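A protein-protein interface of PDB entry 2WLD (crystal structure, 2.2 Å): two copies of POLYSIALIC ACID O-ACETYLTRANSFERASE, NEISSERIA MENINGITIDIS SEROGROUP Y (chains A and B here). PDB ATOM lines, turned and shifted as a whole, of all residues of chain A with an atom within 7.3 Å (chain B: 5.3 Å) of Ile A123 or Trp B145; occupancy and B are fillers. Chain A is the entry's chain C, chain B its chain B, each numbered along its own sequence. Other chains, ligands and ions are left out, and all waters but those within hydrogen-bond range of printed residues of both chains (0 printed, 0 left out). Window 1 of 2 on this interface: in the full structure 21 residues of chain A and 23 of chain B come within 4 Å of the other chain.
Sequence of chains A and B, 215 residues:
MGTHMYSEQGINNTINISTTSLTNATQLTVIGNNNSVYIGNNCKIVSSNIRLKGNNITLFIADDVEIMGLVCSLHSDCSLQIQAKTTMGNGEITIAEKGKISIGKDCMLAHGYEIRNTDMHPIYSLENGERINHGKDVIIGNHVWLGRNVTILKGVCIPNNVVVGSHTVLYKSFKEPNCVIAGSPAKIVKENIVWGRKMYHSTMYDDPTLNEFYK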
ATOM      1  N   ARG A 116      34.906   6.828  -3.523  1.00  0.00           N
ATOM      2  CA  ARG A 116      34.861   8.102  -4.216  1.00  0.00           C
ATOM      3  C   ARG A 116      34.358   9.241  -3.358  1.00  0.00           C
ATOM      4  O   ARG A 116      33.653   9.047  -2.364  1.00  0.00           O
ATOM      5  CB  ARG A 116      34.003   7.973  -5.466  1.00  0.00           C
ATOM      6  CG  ARG A 116      32.627   7.477  -5.182  1.00  0.00           C
ATOM      7  CD  ARG A 116      31.924   6.974  -6.434  1.00  0.00           C
ATOM      8  NE  ARG A 116      30.542   6.758  -6.070  1.00  0.00           N
ATOM      9  CZ  ARG A 116      29.645   6.143  -6.821  1.00  0.00           C
ATOM     10  NH1 ARG A 116      28.403   5.999  -6.370  1.00  0.00           N
ATOM     11  NH2 ARG A 116      29.981   5.680  -8.025  1.00  0.00           N
ATOM     12  N   ASP A 119      29.533  12.140  -6.471  1.00  0.00           N
ATOM     13  CA  ASP A 119      28.465  11.401  -7.100  1.00  0.00           C
ATOM     14  C   ASP A 119      28.635  11.431  -8.630  1.00  0.00           C
ATOM     15  O   ASP A 119      27.902  10.762  -9.351  1.00  0.00           O
ATOM     16  CB  ASP A 119      27.115  12.006  -6.714  1.00  0.00           C
ATOM     17  CG  ASP A 119      26.795  11.863  -5.235  1.00  0.00           C
ATOM     18  OD1 ASP A 119      27.356  10.973  -4.574  1.00  0.00           O
ATOM     19  OD2 ASP A 119      25.965  12.641  -4.727  1.00  0.00           O
ATOM     20  N   MET A 120      29.584  12.228  -9.114  1.00  0.00           N
ATOM     21  CA  MET A 120      29.874  12.373 -10.562  1.00  0.00           C
ATOM     22  C   MET A 120      28.823  13.165 -11.350  1.00  0.00           C
ATOM     23  O   MET A 120      29.057  13.603 -12.477  1.00  0.00           O
ATOM     24  CB  MET A 120      30.117  11.006 -11.202  1.00  0.00           C
ATOM     25  CG  MET A 120      31.520  10.448 -10.899  1.00  0.00           C
ATOM     26  SD  MET A 120      32.791  11.696 -11.280  1.00  0.00           S
ATOM     27  CE  MET A 120      33.149  11.274 -13.000  1.00  0.00           C
ATOM     28  N   HIS A 121      27.671  13.377 -10.741  1.00  0.00           N
ATOM     29  CA  HIS A 121      26.592  14.027 -11.432  1.00  0.00           C
ATOM     30  C   HIS A 121      25.791  14.818 -10.411  1.00  0.00           C
ATOM     31  O   HIS A 121      25.623  14.373  -9.279  1.00  0.00           O
ATOM     32  CB  HIS A 121      25.741  12.982 -12.182  1.00  0.00           C
ATOM     33  CG  HIS A 121      26.536  12.104 -13.108  1.00  0.00           C
ATOM     34  ND1 HIS A 121      26.960  12.518 -14.355  1.00  0.00           N
ATOM     35  CD2 HIS A 121      26.976  10.828 -12.968  1.00  0.00           C
ATOM     36  CE1 HIS A 121      27.637  11.543 -14.936  1.00  0.00           C
ATOM     37  NE2 HIS A 121      27.661  10.505 -14.116  1.00  0.00           N
ATOM     38  N   PRO A 122      25.314  16.007 -10.802  1.00  0.00           N
ATOM     39  CA  PRO A 122      24.681  16.906  -9.860  1.00  0.00           C
ATOM     40  C   PRO A 122      23.258  16.514  -9.543  1.00  0.00           C
ATOM     41  O   PRO A 122      22.549  15.974 -10.412  1.00  0.00           O
ATOM     42  CB  PRO A 122      24.685  18.240 -10.599  1.00  0.00           C
ATOM     43  CG  PRO A 122      24.486  17.824 -12.049  1.00  0.00           C
ATOM     44  CD  PRO A 122      25.266  16.522 -12.177  1.00  0.00           C
ATOM     45  N   ILE A 123      22.872  16.754  -8.287  1.00  0.00           N
ATOM     46  CA  ILE A 123      21.477  16.738  -7.863  1.00  0.00           C
ATOM     47  C   ILE A 123      21.076  18.149  -7.392  1.00  0.00           C
ATOM     48  O   ILE A 123      21.747  18.724  -6.555  1.00  0.00           O
ATOM     49  CB  ILE A 123      21.258  15.744  -6.727  1.00  0.00           C
ATOM     50  CG1 ILE A 123      21.598  14.319  -7.184  1.00  0.00           C
ATOM     51  CG2 ILE A 123      19.813  15.804  -6.282  1.00  0.00           C
ATOM     52  CD1 ILE A 123      21.469  13.272  -6.089  1.00  0.00           C
ATOM     53  N   TYR A 124      19.999  18.713  -7.923  1.00  0.00           N
ATOM     54  CA  TYR A 124      19.586  20.070  -7.568  1.00  0.00           C
ATOM     55  C   TYR A 124      18.265  20.064  -6.791  1.00  0.00           C
ATOM     56  O   TYR A 124      17.422  19.174  -6.972  1.00  0.00           O
ATOM     57  CB  TYR A 124      19.374  20.920  -8.813  1.00  0.00           C
ATOM     58  CG  TYR A 124      20.418  20.845  -9.901  1.00  0.00           C
ATOM     59  CD1 TYR A 124      21.513  21.704  -9.917  1.00  0.00           C
ATOM     60  CD2 TYR A 124      20.267  19.968 -10.960  1.00  0.00           C
ATOM     61  CE1 TYR A 124      22.448  21.647 -10.953  1.00  0.00           C
ATOM     62  CE2 TYR A 124      21.190  19.900 -11.989  1.00  0.00           C
ATOM     63  CZ  TYR A 124      22.272  20.733 -11.984  1.00  0.00           C
ATOM     64  OH  TYR A 124      23.167  20.647 -13.023  1.00  0.00           O
ATOM     65  N   SER A 125      18.068  21.079  -5.954  1.00  0.00           N
ATOM     66  CA  SER A 125      16.787  21.276  -5.263  1.00  0.00           C
ATOM     67  C   SER A 125      15.755  21.925  -6.186  1.00  0.00           C
ATOM     68  O   SER A 125      16.060  22.886  -6.892  1.00  0.00           O
ATOM     69  CB  SER A 125      16.949  22.160  -4.013  1.00  0.00           C
ATOM     70  OG  SER A 125      15.682  22.507  -3.476  1.00  0.00           O
ATOM     71  N   GLY A 129      16.749  25.578  -7.197  1.00  0.00           N
ATOM     72  CA  GLY A 129      17.580  25.201  -8.347  1.00  0.00           C
ATOM     73  C   GLY A 129      19.043  24.938  -8.017  1.00  0.00           C
ATOM     74  O   GLY A 129      19.867  24.647  -8.909  1.00  0.00           O
ATOM     75  N   GLU A 130      19.363  25.053  -6.734  1.00  0.00           N
ATOM     76  CA  GLU A 130      20.733  24.930  -6.268  1.00  0.00           C
ATOM     77  C   GLU A 130      21.168  23.461  -6.204  1.00  0.00           C
ATOM     78  O   GLU A 130      20.344  22.574  -5.978  1.00  0.00           O
ATOM     79  CB  GLU A 130      20.882  25.583  -4.889  1.00  0.00           C
ATOM     80  CG  GLU A 130      20.592  27.087  -4.875  1.00  0.00           C
ATOM     81  CD  GLU A 130      21.050  27.758  -6.152  1.00  0.00           C
ATOM     82  OE1 GLU A 130      22.272  27.760  -6.421  1.00  0.00           O
ATOM     83  OE2 GLU A 130      20.185  28.270  -6.894  1.00  0.00           O
ATOM     84  N   ARG A 131      22.461  23.228  -6.420  1.00  0.00           N
ATOM     85  CA  ARG A 131      23.080  21.905  -6.218  1.00  0.00           C
ATOM     86  C   ARG A 131      23.151  21.516  -4.724  1.00  0.00           C
ATOM     87  O   ARG A 131      23.612  22.288  -3.908  1.00  0.00           O
ATOM     88  CB  ARG A 131      24.491  21.890  -6.824  1.00  0.00           C
ATOM     89  CG  ARG A 131      25.078  20.484  -6.879  1.00  0.00           C
ATOM     90  CD  ARG A 131      26.462  20.365  -7.541  1.00  0.00           C
ATOM     91  NE  ARG A 131      26.917  18.984  -7.437  1.00  0.00           N
ATOM     92  CZ  ARG A 131      28.130  18.544  -7.751  1.00  0.00           C
ATOM     93  NH1 ARG A 131      29.049  19.368  -8.222  1.00  0.00           N
ATOM     94  NH2 ARG A 131      28.408  17.266  -7.607  1.00  0.00           N
ATOM     95  N   ILE A 132      22.697  20.324  -4.359  1.00  0.00           N
ATOM     96  CA  ILE A 132      22.760  19.922  -2.949  1.00  0.00           C
ATOM     97  C   ILE A 132      23.635  18.688  -2.653  1.00  0.00           C
ATOM     98  O   ILE A 132      23.743  18.264  -1.491  1.00  0.00           O
ATOM     99  CB  ILE A 132      21.338  19.727  -2.369  1.00  0.00           C
ATOM    100  CG1 ILE A 132      20.459  18.880  -3.292  1.00  0.00           C
ATOM    101  CG2 ILE A 132      20.650  21.080  -2.235  1.00  0.00           C
ATOM    102  CD1 ILE A 132      20.684  17.450  -3.217  1.00  0.00           C
ATOM    103  N   ASN A 133      24.274  18.131  -3.685  1.00  0.00           N
ATOM    104  CA  ASN A 133      25.168  16.968  -3.518  1.00  0.00           C
ATOM    105  C   ASN A 133      26.649  17.213  -3.900  1.00  0.00           C
ATOM    106  O   ASN A 133      27.259  16.433  -4.638  1.00  0.00           O
ATOM    107  CB  ASN A 133      24.647  15.768  -4.306  1.00  0.00           C
ATOM    108  CG  ASN A 133      24.897  15.892  -5.801  1.00  0.00           C
ATOM    109  OD1 ASN A 133      24.977  16.996  -6.338  1.00  0.00           O
ATOM    110  ND2 ASN A 133      24.981  14.748  -6.488  1.00  0.00           N
ATOM    111  N   HIS A 134      27.229  18.273  -3.368  1.00  0.00           N
ATOM    112  CA  HIS A 134      28.630  18.609  -3.624  1.00  0.00           C
ATOM    113  C   HIS A 134      29.581  17.521  -3.095  1.00  0.00           C
ATOM    114  O   HIS A 134      29.316  16.904  -2.061  1.00  0.00           O
ATOM    115  CB  HIS A 134      28.973  19.939  -2.954  1.00  0.00           C
ATOM    116  CG  HIS A 134      28.419  21.139  -3.656  1.00  0.00           C
ATOM    117  ND1 HIS A 134      29.019  21.698  -4.769  1.00  0.00           N
ATOM    118  CD2 HIS A 134      27.344  21.918  -3.378  1.00  0.00           C
ATOM    119  CE1 HIS A 134      28.323  22.753  -5.157  1.00  0.00           C
ATOM    120  NE2 HIS A 134      27.309  22.914  -4.324  1.00  0.00           N
ATOM    121  N   LYS A 154      31.032   9.685  -0.541  1.00  0.00           N
ATOM    122  CA  LYS A 154      31.619  10.989  -0.296  1.00  0.00           C
ATOM    123  C   LYS A 154      31.466  11.361   1.169  1.00  0.00           C
ATOM    124  O   LYS A 154      30.503  10.972   1.820  1.00  0.00           O
ATOM    125  CB  LYS A 154      31.003  12.036  -1.237  1.00  0.00           C
ATOM    126  CG  LYS A 154      29.529  12.312  -0.981  1.00  0.00           C
ATOM    127  CD  LYS A 154      28.955  13.255  -2.051  1.00  0.00           C
ATOM    128  CE  LYS A 154      27.538  13.693  -1.710  1.00  0.00           C
ATOM    129  NZ  LYS A 154      26.504  12.743  -2.167  1.00  0.00           N
ATOM    130  N   MET B 108      19.846   7.568 -16.983  1.00  0.00           N
ATOM    131  CA  MET B 108      21.267   7.306 -16.827  1.00  0.00           C
ATOM    132  C   MET B 108      21.450   6.101 -15.906  1.00  0.00           C
ATOM    133  O   MET B 108      21.274   6.200 -14.686  1.00  0.00           O
ATOM    134  CB  MET B 108      21.945   8.546 -16.251  1.00  0.00           C
ATOM    135  CG  MET B 108      23.455   8.536 -16.280  1.00  0.00           C
ATOM    136  SD  MET B 108      24.128  10.105 -15.713  1.00  0.00           S
ATOM    137  CE  MET B 108      23.378  10.268 -14.086  1.00  0.00           C
ATOM    138  N   ALA B 110      23.900   3.475 -14.337  1.00  0.00           N
ATOM    139  CA  ALA B 110      25.295   3.242 -14.005  1.00  0.00           C
ATOM    140  C   ALA B 110      25.600   1.759 -13.966  1.00  0.00           C
ATOM    141  O   ALA B 110      24.715   0.919 -13.782  1.00  0.00           O
ATOM    142  CB  ALA B 110      25.637   3.892 -12.639  1.00  0.00           C
ATOM    143  N   HIS B 143      13.751  10.142 -17.181  1.00  0.00           N
ATOM    144  CA  HIS B 143      14.768  10.803 -16.378  1.00  0.00           C
ATOM    145  C   HIS B 143      14.951  10.095 -15.034  1.00  0.00           C
ATOM    146  O   HIS B 143      14.749  10.689 -13.973  1.00  0.00           O
ATOM    147  CB  HIS B 143      14.378  12.264 -16.164  1.00  0.00           C
ATOM    148  CG  HIS B 143      15.527  13.154 -15.805  1.00  0.00           C
ATOM    149  ND1 HIS B 143      16.506  13.501 -16.707  1.00  0.00           N
ATOM    150  CD2 HIS B 143      15.846  13.776 -14.646  1.00  0.00           C
ATOM    151  CE1 HIS B 143      17.385  14.289 -16.118  1.00  0.00           C
ATOM    152  NE2 HIS B 143      17.014  14.462 -14.864  1.00  0.00           N
ATOM    153  N   VAL B 144      15.311   8.813 -15.099  1.00  0.00           N
ATOM    154  CA  VAL B 144      15.635   8.028 -13.908  1.00  0.00           C
ATOM    155  C   VAL B 144      17.126   7.759 -13.864  1.00  0.00           C
ATOM    156  O   VAL B 144      17.731   7.364 -14.847  1.00  0.00           O
ATOM    157  CB  VAL B 144      14.849   6.693 -13.844  1.00  0.00           C
ATOM    158  CG1 VAL B 144      15.514   5.696 -12.902  1.00  0.00           C
ATOM    159  CG2 VAL B 144      13.451   6.947 -13.360  1.00  0.00           C
ATOM    160  N   TRP B 145      17.718   8.016 -12.712  1.00  0.00           N
ATOM    161  CA  TRP B 145      19.141   7.769 -12.517  1.00  0.00           C
ATOM    162  C   TRP B 145      19.310   6.633 -11.515  1.00  0.00           C
ATOM    163  O   TRP B 145      18.916   6.748 -10.335  1.00  0.00           O
ATOM    164  CB  TRP B 145      19.835   9.053 -12.051  1.00  0.00           C
ATOM    165  CG  TRP B 145      21.260   8.871 -11.645  1.00  0.00           C
ATOM    166  CD1 TRP B 145      22.041   7.787 -11.885  1.00  0.00           C
ATOM    167  CD2 TRP B 145      22.081   9.809 -10.941  1.00  0.00           C
ATOM    168  NE1 TRP B 145      23.291   7.981 -11.368  1.00  0.00           N
ATOM    169  CE2 TRP B 145      23.341   9.209 -10.767  1.00  0.00           C
ATOM    170  CE3 TRP B 145      21.874  11.104 -10.439  1.00  0.00           C
ATOM    171  CZ2 TRP B 145      24.389   9.844 -10.099  1.00  0.00           C
ATOM    172  CZ3 TRP B 145      22.911  11.730  -9.787  1.00  0.00           C
ATOM    173  CH2 TRP B 145      24.161  11.108  -9.625  1.00  0.00           C
ATOM    174  N   LEU B 146      19.858   5.526 -12.006  1.00  0.00           N
ATOM    175  CA  LEU B 146      20.188   4.370 -11.176  1.00  0.00           C
ATOM    176  C   LEU B 146      21.671   4.463 -10.909  1.00  0.00           C
ATOM    177  O   LEU B 146      22.468   4.451 -11.861  1.00  0.00           O
ATOM    178  CB  LEU B 146      19.909   3.054 -11.897  1.00  0.00           C
ATOM    179  CG  LEU B 146      18.483   2.700 -12.325  1.00  0.00           C
ATOM    180  CD1 LEU B 146      18.410   1.241 -12.768  1.00  0.00           C
ATOM    181  CD2 LEU B 146      17.498   2.955 -11.213  1.00  0.00           C
ATOM    182  N   GLY B 147      22.035   4.585  -9.628  1.00  0.00           N
ATOM    183  CA  GLY B 147      23.426   4.559  -9.239  1.00  0.00           C
ATOM    184  C   GLY B 147      23.997   3.171  -9.434  1.00  0.00           C
ATOM    185  O   GLY B 147      23.282   2.237  -9.778  1.00  0.00           O
ATOM    186  N   VAL B 162      13.663  10.345 -10.788  1.00  0.00           N
ATOM    187  CA  VAL B 162      13.961   9.716  -9.512  1.00  0.00           C
ATOM    188  C   VAL B 162      15.408   9.296  -9.590  1.00  0.00           C
ATOM    189  O   VAL B 162      15.887   8.943 -10.667  1.00  0.00           O
ATOM    190  CB  VAL B 162      13.053   8.482  -9.284  1.00  0.00           C
ATOM    191  CG1 VAL B 162      13.598   7.557  -8.185  1.00  0.00           C
ATOM    192  CG2 VAL B 162      11.646   8.930  -8.964  1.00  0.00           C
ATOM    193  N   VAL B 163      16.104   9.361  -8.465  1.00  0.00           N
ATOM    194  CA  VAL B 163      17.471   8.875  -8.355  1.00  0.00           C
ATOM    195  C   VAL B 163      17.424   7.691  -7.416  1.00  0.00           C
ATOM    196  O   VAL B 163      16.797   7.762  -6.362  1.00  0.00           O
ATOM    197  CB  VAL B 163      18.412   9.908  -7.685  1.00  0.00           C
ATOM    198  CG1 VAL B 163      19.875   9.413  -7.703  1.00  0.00           C
ATOM    199  CG2 VAL B 163      18.288  11.261  -8.328  1.00  0.00           C
ATOM    200  N   VAL B 164      18.093   6.610  -7.778  1.00  0.00           N
ATOM    201  CA  VAL B 164      18.168   5.450  -6.902  1.00  0.00           C
ATOM    202  C   VAL B 164      19.617   5.300  -6.467  1.00  0.00           C
ATOM    203  O   VAL B 164      20.527   5.211  -7.297  1.00  0.00           O
ATOM    204  CB  VAL B 164      17.666   4.169  -7.589  1.00  0.00           C
ATOM    205  CG1 VAL B 164      17.756   2.995  -6.640  1.00  0.00           C
ATOM    206  CG2 VAL B 164      16.215   4.349  -8.094  1.00  0.00           C
ATOM    207  N   VAL B 180      14.771  10.962  -4.077  1.00  0.00           N
ATOM    208  CA  VAL B 180      15.894  10.045  -4.090  1.00  0.00           C
ATOM    209  C   VAL B 180      15.494   8.867  -3.252  1.00  0.00           C
ATOM    210  O   VAL B 180      14.841   9.035  -2.215  1.00  0.00           O
ATOM    211  CB  VAL B 180      17.174  10.663  -3.511  1.00  0.00           C
ATOM    212  CG1 VAL B 180      18.268   9.605  -3.400  1.00  0.00           C
ATOM    213  CG2 VAL B 180      17.625  11.847  -4.355  1.00  0.00           C
ATOM    214  N   ILE B 193      13.743  17.126  -5.702  1.00  0.00           N
ATOM    215  CA  ILE B 193      15.001  17.331  -6.397  1.00  0.00           C
ATOM    216  C   ILE B 193      14.885  17.024  -7.876  1.00  0.00           C
ATOM    217  O   ILE B 193      13.869  16.511  -8.350  1.00  0.00           O
ATOM    218  CB  ILE B 193      16.107  16.448  -5.815  1.00  0.00           C
ATOM    219  CG1 ILE B 193      15.699  14.972  -5.851  1.00  0.00           C
ATOM    220  CG2 ILE B 193      16.417  16.879  -4.388  1.00  0.00           C
ATOM    221  CD1 ILE B 193      15.768  14.329  -7.234  1.00  0.00           C
ATOM    222  N   VAL B 194      15.939  17.381  -8.596  1.00  0.00           N
ATOM    223  CA  VAL B 194      16.068  17.058  -9.995  1.00  0.00           C
ATOM    224  C   VAL B 194      17.556  16.825 -10.243  1.00  0.00           C
ATOM    225  O   VAL B 194      18.394  17.620  -9.800  1.00  0.00           O
ATOM    226  CB  VAL B 194      15.468  18.155 -10.917  1.00  0.00           C
ATOM    227  CG1 VAL B 194      16.184  19.489 -10.754  1.00  0.00           C
ATOM    228  CG2 VAL B 194      15.509  17.707 -12.375  1.00  0.00           C
ATOM    229  N   TRP B 195      17.884  15.700 -10.885  1.00  0.00           N
ATOM    230  CA  TRP B 195      19.275  15.395 -11.198  1.00  0.00           C
ATOM    231  C   TRP B 195      19.625  15.813 -12.605  1.00  0.00           C
ATOM    232  O   TRP B 195      18.749  15.953 -13.468  1.00  0.00           O
ATOM    233  CB  TRP B 195      19.573  13.905 -11.014  1.00  0.00           C
ATOM    234  CG  TRP B 195      18.849  13.020 -11.953  1.00  0.00           C
ATOM    235  CD1 TRP B 195      17.625  12.449 -11.760  1.00  0.00           C
ATOM    236  CD2 TRP B 195      19.320  12.552 -13.231  1.00  0.00           C
ATOM    237  NE1 TRP B 195      17.292  11.676 -12.848  1.00  0.00           N
ATOM    238  CE2 TRP B 195      18.314  11.722 -13.765  1.00  0.00           C
ATOM    239  CE3 TRP B 195      20.484  12.776 -13.981  1.00  0.00           C
ATOM    240  CZ2 TRP B 195      18.434  11.108 -15.021  1.00  0.00           C
ATOM    241  CZ3 TRP B 195      20.609  12.173 -15.210  1.00  0.00           C
ATOM    242  CH2 TRP B 195      19.586  11.341 -15.728  1.00  0.00           C
ATOM    243  N   GLY B 196      20.910  16.030 -12.845  1.00  0.00           N
ATOM    244  CA  GLY B 196      21.375  16.330 -14.193  1.00  0.00           C
ATOM    245  C   GLY B 196      22.630  15.548 -14.480  1.00  0.00           C
ATOM    246  O   GLY B 196      23.152  14.884 -13.598  1.00  0.00           O
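Among the printed residues, merely in contact across the chains: Tyr A124 with Ile B193, Pro A122 with Trp B195, His A121 with Gly B196, His A121 with Trp B145, Ile A123 with Val B194, Asp A119 with Trp B145, His A121 with Met B108, Ile A123 with Ile B193, Ile A123 with Trp B145 and Tyr A124 with Gly B196.
Ile A123 touches just these residues of chain B: Trp B145 (3.9 Å), Ile B193 (3.8 Å) and Val B194 (3.6 Å).
Of the printed residues of chain A, Trp B145 touches Asp A119 (3.7 Å), His A121 (3.5 Å) and Ile A123 (3.9 Å).
Of the printed residues of chain A, Met B108 touches His A121 (3.8 Å).
Of the printed residues of chain B, Pro A122 touches Trp B195 and Gly B196.
Of the printed residues of chain A, Gly B196 touches His A121, Pro A122 and Tyr A124.
Of the printed residues of chain B, Asp A119 touches Trp B145.
His A134 touches none of the printed residues of chain B.
Ile A132 touches none of the printed residues of chain B.
Of the 15 printed residues of chain B, 6 touch a printed residue of chain A.
Of the 15 printed residues of chain A, 5 touch a printed residue of chain B.
Hydrophobic or aromatic side chains of chain A that line the printed part of chain B: His A121, Pro A122, Ile A123 and Tyr A124.
No position is printed for both chains.
The backbone carbonyl oxygen of Val B194 is in hydrogen-bond range of the backbone NH of Tyr A124 (2.7 Å).
O of Pro A122 sits at hydrogen-bond distance from N of Gly B196, at 2.9 Å.
The backbone carbonyl oxygen (O) of Val B144 is in hydrogen-bond range of the backbone NH (N) of Met B108.
A ring nitrogen (NE2) of His B143 sits at hydrogen-bond distance from the backbone carbonyl oxygen of Trp B195, 2.7 Å away.
The backbone NH (N) of Trp B145 lies within hydrogen-bond range of the backbone carbonyl oxygen (O) of Val B162.
O of Trp B145 lies within hydrogen-bond range of N of Val B164 (2.7 Å).
The side-chain carboxylate (OD2) of Asp A119 lies within salt-bridge range of the side-chain amino group (NZ) of Lys A154, at 2.6 Å.
The side-chain amide nitrogen of Asn A133 is in hydrogen-bond range of the backbone carbonyl oxygen of His A121.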
